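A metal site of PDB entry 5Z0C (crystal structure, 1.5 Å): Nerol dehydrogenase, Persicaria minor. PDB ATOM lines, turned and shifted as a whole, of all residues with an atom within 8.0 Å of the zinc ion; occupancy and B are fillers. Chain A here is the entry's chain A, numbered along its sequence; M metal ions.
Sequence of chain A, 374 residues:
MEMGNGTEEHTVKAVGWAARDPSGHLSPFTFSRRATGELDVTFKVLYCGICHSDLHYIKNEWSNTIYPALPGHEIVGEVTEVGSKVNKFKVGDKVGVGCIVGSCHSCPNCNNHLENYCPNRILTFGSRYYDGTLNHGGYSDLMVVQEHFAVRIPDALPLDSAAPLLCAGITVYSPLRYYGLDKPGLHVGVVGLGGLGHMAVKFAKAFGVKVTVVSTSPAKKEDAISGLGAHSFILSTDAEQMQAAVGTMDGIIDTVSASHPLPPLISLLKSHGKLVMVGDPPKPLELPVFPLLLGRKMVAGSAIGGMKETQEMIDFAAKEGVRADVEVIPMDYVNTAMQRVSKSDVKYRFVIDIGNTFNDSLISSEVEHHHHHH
N of His 105 lies close to SG of Cys 110 (3.4 Å).
The side-chain sulfur of Cys 118 sits close to the backbone NH of Arg 121, 3.7 Å away.
N of Asn 120 lies close to SG of Cys 118 (3.2 Å).
The side-chain amide nitrogen (ND2) of Asn 111 lies close to the backbone carbonyl oxygen (O) of Cys 107 (3.3 Å).
The side-chain sulfur (SG) of Cys 107 lies close to the backbone NH (N) of Asn 109 (3.6 Å).
The side-chain sulfur of Cys 110 lies close to the side-chain hydroxyl of Ser 103 (3.2 Å).
A ring nitrogen (NE2) of His 105 lies close to the backbone carbonyl oxygen of Ser 103, at 3.4 Å.
SG of Cys 104 sits close to N of Ser 106, 3.4 Å away.
N of His 105 touches the zinc ion, at 3.9 Å.
Five residues have an atom within 4 Å of the zinc ion: Cys 104, His 105, Cys 107, Cys 110 and Cys 118.
Along chain A the residues within 4 Å of the zinc ion span positions 104 to 118.
The nearest printed residue that does not touch the zinc ion is Ser 106 (4.4 Å).
SG of Cys 107 binds the zinc ion (2.3 Å).
SG of Cys 104 is bound to the zinc ion, at 2.3 Å.
The zinc ion is bound by SG of Cys 118 (2.4 Å).
SG of Cys 110 is bound to the zinc ion (2.4 Å).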
ATOM      1  N   GLY A 102      -0.546  12.681   8.167  1.00  0.00           N
ATOM      2  CA  GLY A 102      -1.578  11.664   8.097  1.00  0.00           C
ATOM      3  C   GLY A 102      -1.745  11.214   6.679  1.00  0.00           C
ATOM      4  O   GLY A 102      -1.504  11.986   5.731  1.00  0.00           O
ATOM      5  N   SER A 103      -2.301  10.007   6.546  1.00  0.00           N
ATOM      6  CA  SER A 103      -2.778   9.538   5.230  1.00  0.00           C
ATOM      7  C   SER A 103      -3.667   8.317   5.535  1.00  0.00           C
ATOM      8  O   SER A 103      -3.842   7.911   6.709  1.00  0.00           O
ATOM      9  CB  SER A 103      -1.636   9.145   4.286  1.00  0.00           C
ATOM     10  OG  SER A 103      -0.890   8.015   4.765  1.00  0.00           O
ATOM     11  N   CYS A 104      -4.235   7.732   4.457  1.00  0.00           N
ATOM     12  CA  CYS A 104      -5.274   6.730   4.694  1.00  0.00           C
ATOM     13  C   CYS A 104      -4.858   5.345   5.034  1.00  0.00           C
ATOM     14  O   CYS A 104      -5.683   4.590   5.664  1.00  0.00           O
ATOM     15  CB  CYS A 104      -6.292   6.723   3.526  1.00  0.00           C
ATOM     16  SG  CYS A 104      -5.747   5.722   2.081  1.00  0.00           S
ATOM     17  N   HIS A 105      -3.641   4.971   4.687  1.00  0.00           N
ATOM     18  CA  HIS A 105      -3.020   3.726   4.954  1.00  0.00           C
ATOM     19  C   HIS A 105      -3.744   2.541   4.232  1.00  0.00           C
ATOM     20  O   HIS A 105      -3.552   1.431   4.645  1.00  0.00           O
ATOM     21  CB  HIS A 105      -2.891   3.419   6.426  1.00  0.00           C
ATOM     22  CG  HIS A 105      -2.156   4.487   7.160  1.00  0.00           C
ATOM     23  ND1 HIS A 105      -0.834   4.787   6.898  1.00  0.00           N
ATOM     24  CD2 HIS A 105      -2.560   5.337   8.143  1.00  0.00           C
ATOM     25  CE1 HIS A 105      -0.445   5.774   7.701  1.00  0.00           C
ATOM     26  NE2 HIS A 105      -1.499   6.157   8.416  1.00  0.00           N
ATOM     27  N   SER A 106      -4.557   2.800   3.241  1.00  0.00           N
ATOM     28  CA  SER A 106      -5.234   1.727   2.515  1.00  0.00           C
ATOM     29  C   SER A 106      -5.638   2.245   1.132  1.00  0.00           C
ATOM     30  O   SER A 106      -6.858   2.328   0.756  1.00  0.00           O
ATOM     31  CB  SER A 106      -6.471   1.260   3.242  1.00  0.00           C
ATOM     32  OG  SER A 106      -7.366   2.315   3.246  1.00  0.00           O
ATOM     33  N   CYS A 107      -4.660   2.785   0.436  1.00  0.00           N
ATOM     34  CA  CYS A 107      -4.747   3.078  -0.999  1.00  0.00           C
ATOM     35  C   CYS A 107      -3.435   2.620  -1.640  1.00  0.00           C
ATOM     36  O   CYS A 107      -2.496   2.301  -0.948  1.00  0.00           O
ATOM     37  CB  CYS A 107      -5.087   4.529  -1.281  1.00  0.00           C
ATOM     38  SG  CYS A 107      -3.639   5.695  -1.022  1.00  0.00           S
ATOM     39  N   PRO A 108      -3.404   2.533  -2.999  1.00  0.00           N
ATOM     40  CA  PRO A 108      -2.193   2.054  -3.632  1.00  0.00           C
ATOM     41  C   PRO A 108      -0.983   2.924  -3.345  1.00  0.00           C
ATOM     42  O   PRO A 108       0.085   2.378  -3.154  1.00  0.00           O
ATOM     43  CB  PRO A 108      -2.529   2.111  -5.121  1.00  0.00           C
ATOM     44  CG  PRO A 108      -4.029   1.857  -5.107  1.00  0.00           C
ATOM     45  CD  PRO A 108      -4.521   2.672  -3.961  1.00  0.00           C
ATOM     46  N   ASN A 109      -1.200   4.228  -3.260  1.00  0.00           N
ATOM     47  CA  ASN A 109      -0.048   5.114  -2.910  1.00  0.00           C
ATOM     48  C   ASN A 109       0.470   4.892  -1.482  1.00  0.00           C
ATOM     49  O   ASN A 109       1.664   4.727  -1.290  1.00  0.00           O
ATOM     50  CB  ASN A 109      -0.400   6.526  -3.187  1.00  0.00           C
ATOM     51  CG  ASN A 109      -0.228   6.830  -4.676  1.00  0.00           C
ATOM     52  OD1 ASN A 109       0.801   6.618  -5.179  1.00  0.00           O
ATOM     53  ND2 ASN A 109      -1.237   7.257  -5.326  1.00  0.00           N
ATOM     54  N   CYS A 110      -0.422   4.822  -0.516  1.00  0.00           N
ATOM     55  CA  CYS A 110       0.053   4.520   0.828  1.00  0.00           C
ATOM     56  C   CYS A 110       0.746   3.216   0.881  1.00  0.00           C
ATOM     57  O   CYS A 110       1.783   3.031   1.527  1.00  0.00           O
ATOM     58  CB  CYS A 110      -1.062   4.631   1.857  1.00  0.00           C
ATOM     59  SG  CYS A 110      -1.718   6.294   2.195  1.00  0.00           S
ATOM     60  N   ASN A 111       0.131   2.206   0.225  1.00  0.00           N
ATOM     61  CA  ASN A 111       0.719   0.827   0.266  1.00  0.00           C
ATOM     62  C   ASN A 111       2.046   0.725  -0.398  1.00  0.00           C
ATOM     63  O   ASN A 111       2.819  -0.165  -0.065  1.00  0.00           O
ATOM     64  CB  ASN A 111      -0.210  -0.225  -0.351  1.00  0.00           C
ATOM     65  CG  ASN A 111      -1.531  -0.354   0.368  1.00  0.00           C
ATOM     66  OD1 ASN A 111      -1.676   0.036   1.510  1.00  0.00           O
ATOM     67  ND2 ASN A 111      -2.536  -0.905  -0.331  1.00  0.00           N
ATOM     68  N   LEU A 114       4.039   5.993  -0.410  1.00  0.00           N
ATOM     69  CA  LEU A 114       3.838   7.264  -1.096  1.00  0.00           C
ATOM     70  C   LEU A 114       2.692   7.990  -0.503  1.00  0.00           C
ATOM     71  O   LEU A 114       1.747   8.347  -1.175  1.00  0.00           O
ATOM     72  CB  LEU A 114       3.712   7.050  -2.625  1.00  0.00           C
ATOM     73  CG  LEU A 114       4.979   6.449  -3.219  1.00  0.00           C
ATOM     74  CD1 LEU A 114       4.693   5.914  -4.622  1.00  0.00           C
ATOM     75  CD2 LEU A 114       6.134   7.477  -3.254  1.00  0.00           C
ATOM     76  N   GLU A 115       2.767   8.181   0.810  1.00  0.00           N
ATOM     77  CA  GLU A 115       1.688   8.910   1.531  1.00  0.00           C
ATOM     78  C   GLU A 115       1.519  10.327   1.040  1.00  0.00           C
ATOM     79  O   GLU A 115       0.436  10.899   1.167  1.00  0.00           O
ATOM     80  CB  GLU A 115       1.987   8.860   3.024  1.00  0.00           C
ATOM     81  CG  GLU A 115       2.262   7.506   3.560  1.00  0.00           C
ATOM     82  CD  GLU A 115       3.693   7.029   3.511  1.00  0.00           C
ATOM     83  OE1 GLU A 115       4.037   5.970   4.117  1.00  0.00           O
ATOM     84  OE2 GLU A 115       4.546   7.729   2.884  1.00  0.00           O
ATOM     85  N   ASN A 116       2.607  10.920   0.496  1.00  0.00           N
ATOM     86  CA  ASN A 116       2.483  12.206  -0.113  1.00  0.00           C
ATOM     87  C   ASN A 116       1.575  12.371  -1.370  1.00  0.00           C
ATOM     88  O   ASN A 116       1.165  13.480  -1.720  1.00  0.00           O
ATOM     89  CB  ASN A 116       3.914  12.696  -0.512  1.00  0.00           C
ATOM     90  CG  ASN A 116       4.661  11.716  -1.358  1.00  0.00           C
ATOM     91  OD1 ASN A 116       4.617  10.506  -1.164  1.00  0.00           O
ATOM     92  ND2 ASN A 116       5.487  12.262  -2.281  1.00  0.00           N
ATOM     93  N   TYR A 117       1.225  11.254  -1.988  1.00  0.00           N
ATOM     94  CA  TYR A 117       0.297  11.172  -3.126  1.00  0.00           C
ATOM     95  C   TYR A 117      -1.007  10.473  -2.705  1.00  0.00           C
ATOM     96  O   TYR A 117      -1.841  10.131  -3.536  1.00  0.00           O
ATOM     97  CB  TYR A 117       0.977  10.416  -4.287  1.00  0.00           C
ATOM     98  CG  TYR A 117       2.245  11.143  -4.782  1.00  0.00           C
ATOM     99  CD1 TYR A 117       2.203  12.415  -5.300  1.00  0.00           C
ATOM    100  CD2 TYR A 117       3.500  10.515  -4.690  1.00  0.00           C
ATOM    101  CE1 TYR A 117       3.379  13.066  -5.723  1.00  0.00           C
ATOM    102  CE2 TYR A 117       4.683  11.160  -5.139  1.00  0.00           C
ATOM    103  CZ  TYR A 117       4.595  12.411  -5.657  1.00  0.00           C
ATOM    104  OH  TYR A 117       5.716  13.114  -6.052  1.00  0.00           O
ATOM    105  N   CYS A 118      -1.221  10.262  -1.401  1.00  0.00           N
ATOM    106  CA  CYS A 118      -2.530   9.808  -0.926  1.00  0.00           C
ATOM    107  C   CYS A 118      -3.573  10.893  -1.152  1.00  0.00           C
ATOM    108  O   CYS A 118      -3.424  12.102  -0.783  1.00  0.00           O
ATOM    109  CB  CYS A 118      -2.435   9.528   0.575  1.00  0.00           C
ATOM    110  SG  CYS A 118      -4.049   8.951   1.249  1.00  0.00           S
ATOM    111  N   PRO A 119      -4.722  10.482  -1.746  1.00  0.00           N
ATOM    112  CA  PRO A 119      -5.729  11.475  -1.951  1.00  0.00           C
ATOM    113  C   PRO A 119      -6.287  12.073  -0.638  1.00  0.00           C
ATOM    114  O   PRO A 119      -6.855  13.164  -0.638  1.00  0.00           O
ATOM    115  CB  PRO A 119      -6.884  10.660  -2.614  1.00  0.00           C
ATOM    116  CG  PRO A 119      -6.293   9.470  -3.064  1.00  0.00           C
ATOM    117  CD  PRO A 119      -5.030   9.189  -2.362  1.00  0.00           C
ATOM    118  N   ASN A 120      -6.119  11.303   0.407  1.00  0.00           N
ATOM    119  CA  ASN A 120      -6.545  11.761   1.738  1.00  0.00           C
ATOM    120  C   ASN A 120      -5.367  12.115   2.648  1.00  0.00           C
ATOM    121  O   ASN A 120      -5.488  12.014   3.909  1.00  0.00           O
ATOM    122  CB  ASN A 120      -7.408  10.684   2.386  1.00  0.00           C
ATOM    123  CG  ASN A 120      -8.751  10.619   1.688  1.00  0.00           C
ATOM    124  OD1 ASN A 120      -9.548  11.544   1.751  1.00  0.00           O
ATOM    125  ND2 ASN A 120      -8.901   9.646   0.907  1.00  0.00           N
ATOM    126  N   ARG A 121      -4.264  12.565   2.062  1.00  0.00           N
ATOM    127  CA  ARG A 121      -3.162  12.996   2.892  1.00  0.00           C
ATOM    128  C   ARG A 121      -3.581  14.159   3.763  1.00  0.00           C
ATOM    129  O   ARG A 121      -4.404  14.966   3.352  1.00  0.00           O
ATOM    130  CB  ARG A 121      -1.952  13.379   2.049  1.00  0.00           C
ATOM    131  CG  ARG A 121      -2.202  14.601   1.174  1.00  0.00           C
ATOM    132  CD  ARG A 121      -1.106  14.818   0.119  1.00  0.00           C
ATOM    133  NE  ARG A 121      -1.196  16.182  -0.400  1.00  0.00           N
ATOM    134  CZ  ARG A 121      -0.187  16.843  -1.016  1.00  0.00           C
ATOM    135  NH1 ARG A 121       1.033  16.322  -1.110  1.00  0.00           N
ATOM    136  NH2 ARG A 121      -0.350  18.111  -1.371  1.00  0.00           N
HETATM  137 ZN    ZN M   1      -3.813   6.608   1.116  1.00  0.00          ZN
